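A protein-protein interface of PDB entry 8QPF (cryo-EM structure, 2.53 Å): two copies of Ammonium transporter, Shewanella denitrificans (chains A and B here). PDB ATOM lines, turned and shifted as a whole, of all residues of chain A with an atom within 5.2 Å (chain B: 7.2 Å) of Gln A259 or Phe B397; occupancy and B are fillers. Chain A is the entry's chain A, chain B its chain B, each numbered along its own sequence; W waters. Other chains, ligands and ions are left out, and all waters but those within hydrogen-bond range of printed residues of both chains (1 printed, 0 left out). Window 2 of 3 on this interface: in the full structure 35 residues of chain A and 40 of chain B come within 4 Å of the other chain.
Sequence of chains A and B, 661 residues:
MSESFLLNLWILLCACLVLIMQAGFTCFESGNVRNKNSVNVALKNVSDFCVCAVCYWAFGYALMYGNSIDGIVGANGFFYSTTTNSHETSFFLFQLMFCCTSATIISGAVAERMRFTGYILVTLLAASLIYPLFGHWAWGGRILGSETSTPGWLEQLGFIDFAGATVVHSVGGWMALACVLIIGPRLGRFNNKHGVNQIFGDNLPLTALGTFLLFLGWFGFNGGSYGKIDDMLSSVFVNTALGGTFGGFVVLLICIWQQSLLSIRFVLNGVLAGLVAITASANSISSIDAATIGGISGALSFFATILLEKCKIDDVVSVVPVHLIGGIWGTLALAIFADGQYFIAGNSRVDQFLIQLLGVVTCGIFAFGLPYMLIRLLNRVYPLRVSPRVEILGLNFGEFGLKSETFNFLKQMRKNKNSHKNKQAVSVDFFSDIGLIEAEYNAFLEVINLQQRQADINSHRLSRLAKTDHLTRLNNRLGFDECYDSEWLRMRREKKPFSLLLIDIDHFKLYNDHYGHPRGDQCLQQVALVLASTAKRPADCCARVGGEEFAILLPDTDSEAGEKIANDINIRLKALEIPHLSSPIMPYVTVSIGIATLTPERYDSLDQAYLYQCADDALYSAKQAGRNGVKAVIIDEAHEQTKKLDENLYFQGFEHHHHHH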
ATOM      1  N   TRP A 257      25.607   6.865 -23.639  1.00  0.00           N
ATOM      2  CA  TRP A 257      24.334   6.887 -22.936  1.00  0.00           C
ATOM      3  C   TRP A 257      24.333   7.815 -21.732  1.00  0.00           C
ATOM      4  O   TRP A 257      23.332   7.867 -21.011  1.00  0.00           O
ATOM      5  CB  TRP A 257      23.949   5.471 -22.500  1.00  0.00           C
ATOM      6  CG  TRP A 257      23.715   4.547 -23.651  1.00  0.00           C
ATOM      7  CD1 TRP A 257      22.805   4.703 -24.653  1.00  0.00           C
ATOM      8  CD2 TRP A 257      24.407   3.324 -23.923  1.00  0.00           C
ATOM      9  NE1 TRP A 257      22.885   3.651 -25.534  1.00  0.00           N
ATOM     10  CE2 TRP A 257      23.861   2.791 -25.108  1.00  0.00           C
ATOM     11  CE3 TRP A 257      25.434   2.626 -23.279  1.00  0.00           C
ATOM     12  CZ2 TRP A 257      24.309   1.592 -25.662  1.00  0.00           C
ATOM     13  CZ3 TRP A 257      25.877   1.436 -23.831  1.00  0.00           C
ATOM     14  CH2 TRP A 257      25.315   0.932 -25.010  1.00  0.00           C
ATOM     15  N   GLN A 258      25.427   8.532 -21.488  1.00  0.00           N
ATOM     16  CA  GLN A 258      25.435   9.551 -20.451  1.00  0.00           C
ATOM     17  C   GLN A 258      24.536  10.712 -20.850  1.00  0.00           C
ATOM     18  O   GLN A 258      24.354  11.007 -22.035  1.00  0.00           O
ATOM     19  CB  GLN A 258      26.857  10.051 -20.188  1.00  0.00           C
ATOM     20  CG  GLN A 258      27.761   9.145 -19.331  1.00  0.00           C
ATOM     21  CD  GLN A 258      27.030   8.060 -18.549  1.00  0.00           C
ATOM     22  OE1 GLN A 258      26.299   8.337 -17.593  1.00  0.00           O
ATOM     23  NE2 GLN A 258      27.227   6.811 -18.956  1.00  0.00           N
ATOM     24  N   GLN A 259      23.957  11.359 -19.845  1.00  0.00           N
ATOM     25  CA  GLN A 259      23.004  12.429 -20.092  1.00  0.00           C
ATOM     26  C   GLN A 259      23.708  13.670 -20.624  1.00  0.00           C
ATOM     27  O   GLN A 259      24.929  13.816 -20.521  1.00  0.00           O
ATOM     28  CB  GLN A 259      22.244  12.769 -18.810  1.00  0.00           C
ATOM     29  CG  GLN A 259      23.083  13.450 -17.751  1.00  0.00           C
ATOM     30  CD  GLN A 259      22.253  14.286 -16.796  1.00  0.00           C
ATOM     31  OE1 GLN A 259      22.445  15.496 -16.684  1.00  0.00           O
ATOM     32  NE2 GLN A 259      21.323  13.642 -16.102  1.00  0.00           N
ATOM     33  N   SER A 260      22.919  14.580 -21.189  1.00  0.00           N
ATOM     34  CA  SER A 260      23.443  15.857 -21.644  1.00  0.00           C
ATOM     35  C   SER A 260      23.707  16.770 -20.444  1.00  0.00           C
ATOM     36  O   SER A 260      23.556  16.374 -19.282  1.00  0.00           O
ATOM     37  CB  SER A 260      22.479  16.502 -22.636  1.00  0.00           C
ATOM     38  OG  SER A 260      22.955  17.765 -23.058  1.00  0.00           O
ATOM     39  N   LEU A 261      24.175  17.991 -20.751  1.00  0.00           N
ATOM     40  CA  LEU A 261      24.553  19.082 -19.838  1.00  0.00           C
ATOM     41  C   LEU A 261      25.828  18.770 -19.044  1.00  0.00           C
ATOM     42  O   LEU A 261      26.357  19.642 -18.349  1.00  0.00           O
ATOM     43  CB  LEU A 261      23.389  19.453 -18.895  1.00  0.00           C
ATOM     44  CG  LEU A 261      23.306  20.773 -18.122  1.00  0.00           C
ATOM     45  CD1 LEU A 261      22.935  21.927 -19.033  1.00  0.00           C
ATOM     46  CD2 LEU A 261      22.318  20.650 -16.972  1.00  0.00           C
ATOM     47  N   LEU A 262      26.357  17.559 -19.165  1.00  0.00           N
ATOM     48  CA  LEU A 262      27.667  17.191 -18.644  1.00  0.00           C
ATOM     49  C   LEU A 262      28.522  16.473 -19.675  1.00  0.00           C
ATOM     50  O   LEU A 262      29.743  16.640 -19.671  1.00  0.00           O
ATOM     51  CB  LEU A 262      27.526  16.323 -17.374  1.00  0.00           C
ATOM     52  CG  LEU A 262      26.632  15.080 -17.352  1.00  0.00           C
ATOM     53  CD1 LEU A 262      27.407  13.806 -17.667  1.00  0.00           C
ATOM     54  CD2 LEU A 262      25.970  14.966 -15.987  1.00  0.00           C
ATOM     55  N   SER A 263      27.914  15.690 -20.566  1.00  0.00           N
ATOM     56  CA  SER A 263      28.665  15.000 -21.605  1.00  0.00           C
ATOM     57  C   SER A 263      29.088  15.921 -22.738  1.00  0.00           C
ATOM     58  O   SER A 263      30.047  15.599 -23.452  1.00  0.00           O
ATOM     59  CB  SER A 263      27.844  13.841 -22.178  1.00  0.00           C
ATOM     60  OG  SER A 263      26.768  14.319 -22.963  1.00  0.00           O
ATOM     61  N   ASN B  35      15.098  26.708 -23.496  1.00  0.00           N
ATOM     62  CA  ASN B  35      16.335  26.645 -22.728  1.00  0.00           C
ATOM     63  C   ASN B  35      16.555  25.284 -22.082  1.00  0.00           C
ATOM     64  O   ASN B  35      17.689  24.962 -21.713  1.00  0.00           O
ATOM     65  CB  ASN B  35      16.337  27.734 -21.656  1.00  0.00           C
ATOM     66  CG  ASN B  35      17.382  28.798 -21.911  1.00  0.00           C
ATOM     67  OD1 ASN B  35      18.095  28.758 -22.913  1.00  0.00           O
ATOM     68  ND2 ASN B  35      17.471  29.766 -21.007  1.00  0.00           N
ATOM     69  N   LYS B  36      15.503  24.478 -21.946  1.00  0.00           N
ATOM     70  CA  LYS B  36      15.608  23.131 -21.405  1.00  0.00           C
ATOM     71  C   LYS B  36      16.029  22.106 -22.449  1.00  0.00           C
ATOM     72  O   LYS B  36      16.163  20.926 -22.110  1.00  0.00           O
ATOM     73  CB  LYS B  36      14.273  22.710 -20.789  1.00  0.00           C
ATOM     74  CG  LYS B  36      13.166  22.513 -21.807  1.00  0.00           C
ATOM     75  CD  LYS B  36      11.849  22.180 -21.139  1.00  0.00           C
ATOM     76  CE  LYS B  36      10.812  21.745 -22.157  1.00  0.00           C
ATOM     77  NZ  LYS B  36       9.482  21.532 -21.530  1.00  0.00           N
ATOM     78  N   ASN B  37      16.230  22.519 -23.701  1.00  0.00           N
ATOM     79  CA  ASN B  37      16.611  21.609 -24.769  1.00  0.00           C
ATOM     80  C   ASN B  37      17.794  22.092 -25.595  1.00  0.00           C
ATOM     81  O   ASN B  37      18.220  21.370 -26.502  1.00  0.00           O
ATOM     82  CB  ASN B  37      15.421  21.362 -25.709  1.00  0.00           C
ATOM     83  CG  ASN B  37      14.241  20.733 -25.006  1.00  0.00           C
ATOM     84  OD1 ASN B  37      14.386  19.747 -24.289  1.00  0.00           O
ATOM     85  ND2 ASN B  37      13.063  21.309 -25.200  1.00  0.00           N
ATOM     86  N   ASN B  40      21.164  19.981 -25.409  1.00  0.00           N
ATOM     87  CA  ASN B  40      21.031  18.750 -26.183  1.00  0.00           C
ATOM     88  C   ASN B  40      21.121  19.019 -27.681  1.00  0.00           C
ATOM     89  O   ASN B  40      21.691  18.215 -28.428  1.00  0.00           O
ATOM     90  CB  ASN B  40      19.710  18.060 -25.847  1.00  0.00           C
ATOM     91  CG  ASN B  40      19.664  16.629 -26.332  1.00  0.00           C
ATOM     92  OD1 ASN B  40      18.786  16.254 -27.106  1.00  0.00           O
ATOM     93  ND2 ASN B  40      20.608  15.818 -25.875  1.00  0.00           N
ATOM     94  N   LEU B  43      24.806  19.612 -28.415  1.00  0.00           N
ATOM     95  CA  LEU B  43      25.494  18.324 -28.378  1.00  0.00           C
ATOM     96  C   LEU B  43      25.205  17.502 -29.629  1.00  0.00           C
ATOM     97  O   LEU B  43      26.107  16.848 -30.168  1.00  0.00           O
ATOM     98  CB  LEU B  43      25.088  17.553 -27.121  1.00  0.00           C
ATOM     99  CG  LEU B  43      25.661  16.146 -26.932  1.00  0.00           C
ATOM    100  CD1 LEU B  43      27.178  16.168 -26.890  1.00  0.00           C
ATOM    101  CD2 LEU B  43      25.096  15.501 -25.683  1.00  0.00           C
ATOM    102  N   ARG B 389       7.743  12.461 -19.791  1.00  0.00           N
ATOM    103  CA  ARG B 389       8.375  13.153 -18.671  1.00  0.00           C
ATOM    104  C   ARG B 389       9.711  13.772 -19.079  1.00  0.00           C
ATOM    105  O   ARG B 389      10.103  14.817 -18.547  1.00  0.00           O
ATOM    106  CB  ARG B 389       8.528  12.202 -17.476  1.00  0.00           C
ATOM    107  CG  ARG B 389       9.641  11.167 -17.570  1.00  0.00           C
ATOM    108  CD  ARG B 389       9.906  10.490 -16.227  1.00  0.00           C
ATOM    109  NE  ARG B 389      11.216   9.847 -16.162  1.00  0.00           N
ATOM    110  CZ  ARG B 389      12.379  10.479 -16.055  1.00  0.00           C
ATOM    111  NH1 ARG B 389      12.448  11.797 -15.937  1.00  0.00           N
ATOM    112  NH2 ARG B 389      13.504   9.770 -16.049  1.00  0.00           N
ATOM    113  N   VAL B 390      10.405  13.164 -20.046  1.00  0.00           N
ATOM    114  CA  VAL B 390      11.639  13.745 -20.564  1.00  0.00           C
ATOM    115  C   VAL B 390      11.336  14.987 -21.394  1.00  0.00           C
ATOM    116  O   VAL B 390      12.028  16.007 -21.287  1.00  0.00           O
ATOM    117  CB  VAL B 390      12.419  12.683 -21.363  1.00  0.00           C
ATOM    118  CG1 VAL B 390      13.575  13.299 -22.130  1.00  0.00           C
ATOM    119  CG2 VAL B 390      12.943  11.615 -20.425  1.00  0.00           C
ATOM    120  N   ILE B 392       8.681  16.941 -21.122  1.00  0.00           N
ATOM    121  CA  ILE B 392       8.233  18.000 -20.221  1.00  0.00           C
ATOM    122  C   ILE B 392       9.415  18.574 -19.443  1.00  0.00           C
ATOM    123  O   ILE B 392       9.578  19.797 -19.345  1.00  0.00           O
ATOM    124  CB  ILE B 392       7.119  17.477 -19.292  1.00  0.00           C
ATOM    125  CG1 ILE B 392       5.777  17.474 -20.026  1.00  0.00           C
ATOM    126  CG2 ILE B 392       7.003  18.305 -18.020  1.00  0.00           C
ATOM    127  CD1 ILE B 392       4.883  16.305 -19.683  1.00  0.00           C
ATOM    128  N   LEU B 393      10.274  17.701 -18.906  1.00  0.00           N
ATOM    129  CA  LEU B 393      11.398  18.162 -18.095  1.00  0.00           C
ATOM    130  C   LEU B 393      12.472  18.829 -18.945  1.00  0.00           C
ATOM    131  O   LEU B 393      13.034  19.858 -18.551  1.00  0.00           O
ATOM    132  CB  LEU B 393      11.992  16.994 -17.310  1.00  0.00           C
ATOM    133  CG  LEU B 393      11.306  16.635 -15.991  1.00  0.00           C
ATOM    134  CD1 LEU B 393      11.978  15.430 -15.354  1.00  0.00           C
ATOM    135  CD2 LEU B 393      11.308  17.821 -15.041  1.00  0.00           C
ATOM    136  N   GLY B 394      12.769  18.267 -20.111  1.00  0.00           N
ATOM    137  CA  GLY B 394      13.805  18.810 -20.961  1.00  0.00           C
ATOM    138  C   GLY B 394      14.804  17.762 -21.397  1.00  0.00           C
ATOM    139  O   GLY B 394      15.105  16.830 -20.645  1.00  0.00           O
ATOM    140  N   LEU B 395      15.328  17.903 -22.613  1.00  0.00           N
ATOM    141  CA  LEU B 395      16.275  16.936 -23.150  1.00  0.00           C
ATOM    142  C   LEU B 395      17.706  17.196 -22.697  1.00  0.00           C
ATOM    143  O   LEU B 395      18.596  16.409 -23.032  1.00  0.00           O
ATOM    144  CB  LEU B 395      16.208  16.922 -24.680  1.00  0.00           C
ATOM    145  CG  LEU B 395      15.349  15.842 -25.348  1.00  0.00           C
ATOM    146  CD1 LEU B 395      13.905  15.868 -24.868  1.00  0.00           C
ATOM    147  CD2 LEU B 395      15.399  15.993 -26.853  1.00  0.00           C
ATOM    148  N   ASN B 396      17.946  18.276 -21.950  1.00  0.00           N
ATOM    149  CA  ASN B 396      19.260  18.516 -21.368  1.00  0.00           C
ATOM    150  C   ASN B 396      19.562  17.582 -20.206  1.00  0.00           C
ATOM    151  O   ASN B 396      20.726  17.446 -19.821  1.00  0.00           O
ATOM    152  CB  ASN B 396      19.370  19.959 -20.872  1.00  0.00           C
ATOM    153  CG  ASN B 396      19.335  20.965 -21.991  1.00  0.00           C
ATOM    154  OD1 ASN B 396      19.436  20.611 -23.164  1.00  0.00           O
ATOM    155  ND2 ASN B 396      19.195  22.236 -21.637  1.00  0.00           N
ATOM    156  N   PHE B 397      18.543  16.947 -19.633  1.00  0.00           N
ATOM    157  CA  PHE B 397      18.668  16.241 -18.368  1.00  0.00           C
ATOM    158  C   PHE B 397      18.561  14.731 -18.526  1.00  0.00           C
ATOM    159  O   PHE B 397      18.311  14.032 -17.540  1.00  0.00           O
ATOM    160  CB  PHE B 397      17.633  16.733 -17.333  1.00  0.00           C
ATOM    161  CG  PHE B 397      17.347  18.233 -17.358  1.00  0.00           C
ATOM    162  CD1 PHE B 397      16.482  18.816 -18.291  1.00  0.00           C
ATOM    163  CD2 PHE B 397      17.980  19.065 -16.448  1.00  0.00           C
ATOM    164  CE1 PHE B 397      16.253  20.179 -18.296  1.00  0.00           C
ATOM    165  CE2 PHE B 397      17.752  20.429 -16.450  1.00  0.00           C
ATOM    166  CZ  PHE B 397      16.887  20.985 -17.375  1.00  0.00           C
ATOM    167  N   GLY B 398      18.744  14.214 -19.731  1.00  0.00           N
ATOM    168  CA  GLY B 398      18.785  12.786 -19.970  1.00  0.00           C
ATOM    169  C   GLY B 398      17.499  12.267 -20.590  1.00  0.00           C
ATOM    170  O   GLY B 398      16.457  12.921 -20.593  1.00  0.00           O
ATOM    171  N   GLU B 399      17.601  11.051 -21.116  1.00  0.00           N
ATOM    172  CA  GLU B 399      16.480  10.390 -21.773  1.00  0.00           C
ATOM    173  C   GLU B 399      16.243   9.003 -21.186  1.00  0.00           C
ATOM    174  O   GLU B 399      16.189   8.834 -19.967  1.00  0.00           O
ATOM    175  CB  GLU B 399      16.726  10.288 -23.279  1.00  0.00           C
ATOM    176  CG  GLU B 399      16.734  11.627 -23.997  1.00  0.00           C
ATOM    177  CD  GLU B 399      17.739  11.675 -25.128  1.00  0.00           C
ATOM    178  OE1 GLU B 399      18.246  10.603 -25.517  1.00  0.00           O
ATOM    179  OE2 GLU B 399      18.022  12.785 -25.625  1.00  0.00           O
HETATM  180  O   HOH W   1      20.092  13.855 -22.859  1.00  0.00           O
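Gln A259 touches just these residues of chain B: Phe B397 and Gly B398.
Printed residues of chain B within 4 Å of Leu A261: Asn B396 (3.5 Å).
Leu A262 touches none of the printed residues of chain B.
Printed residues of chain A within 4 Å of Asn B40: Ser A260 (3.7 Å).
Printed residues of chain A within 4 Å of Leu B43: Ser A263.
Of the printed residues of chain A, Leu B395 touches Ser A260 (3.9 Å).
Phe B397 touches one residue of chain A.
The nearest residue of chain B that does not touch Gln A259 is Asn B396 (4.1 Å).
O of Lys B36 is in hydrogen-bond range of N of Leu B395.
The backbone carbonyl oxygen (O) of Lys B36 lies close to the backbone NH (N) of Asn B396, at 3.2 Å.
The side-chain amide oxygen (OD1) of Asn B396 is in hydrogen-bond range of the backbone NH (N) of Asn B40.
OG of Ser A263 is in hydrogen-bond range of O of Gln A259, at 3.1 Å.
The side-chain amide oxygen (OD1) of Asn B37 is in hydrogen-bond range of the backbone NH (N) of Leu B395.
The backbone carbonyl oxygen (O) of Asn B35 lies within hydrogen-bond range of the side-chain amide nitrogen (ND2) of Asn B396.
Printed residues of chain A that touch a printed residue of chain B: Gln A259, Ser A260, Leu A261 and Ser A263.
Hydrophobic or aromatic side chains of chain A that line the printed part of chain B: Leu A261.
Among the printed residues, 7 pairs touch across the chains.
Water W1 lies within hydrogen-bond range of O of Leu B395 (3.0 Å), N of Ser A260 (3.4 Å) and N of Gly B398 (3.4 Å).
The backbone carbonyl oxygen (O) of Asn B396 lies close to the backbone carbonyl oxygen (O) of Ser A260, 3.1 Å away.
The side-chain amide nitrogen of Gln A259 sits at hydrogen-bond distance from the backbone carbonyl oxygen of Phe B397, at 3.4 Å.
Among the printed residues, merely in contact across the chains: Ser A263 with Leu B43, Leu A261 with Asn B396, Gln A259 with Gly B398, Ser A260 with Asn B40 and Ser A260 with Leu B395.
No position is printed for both chains.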
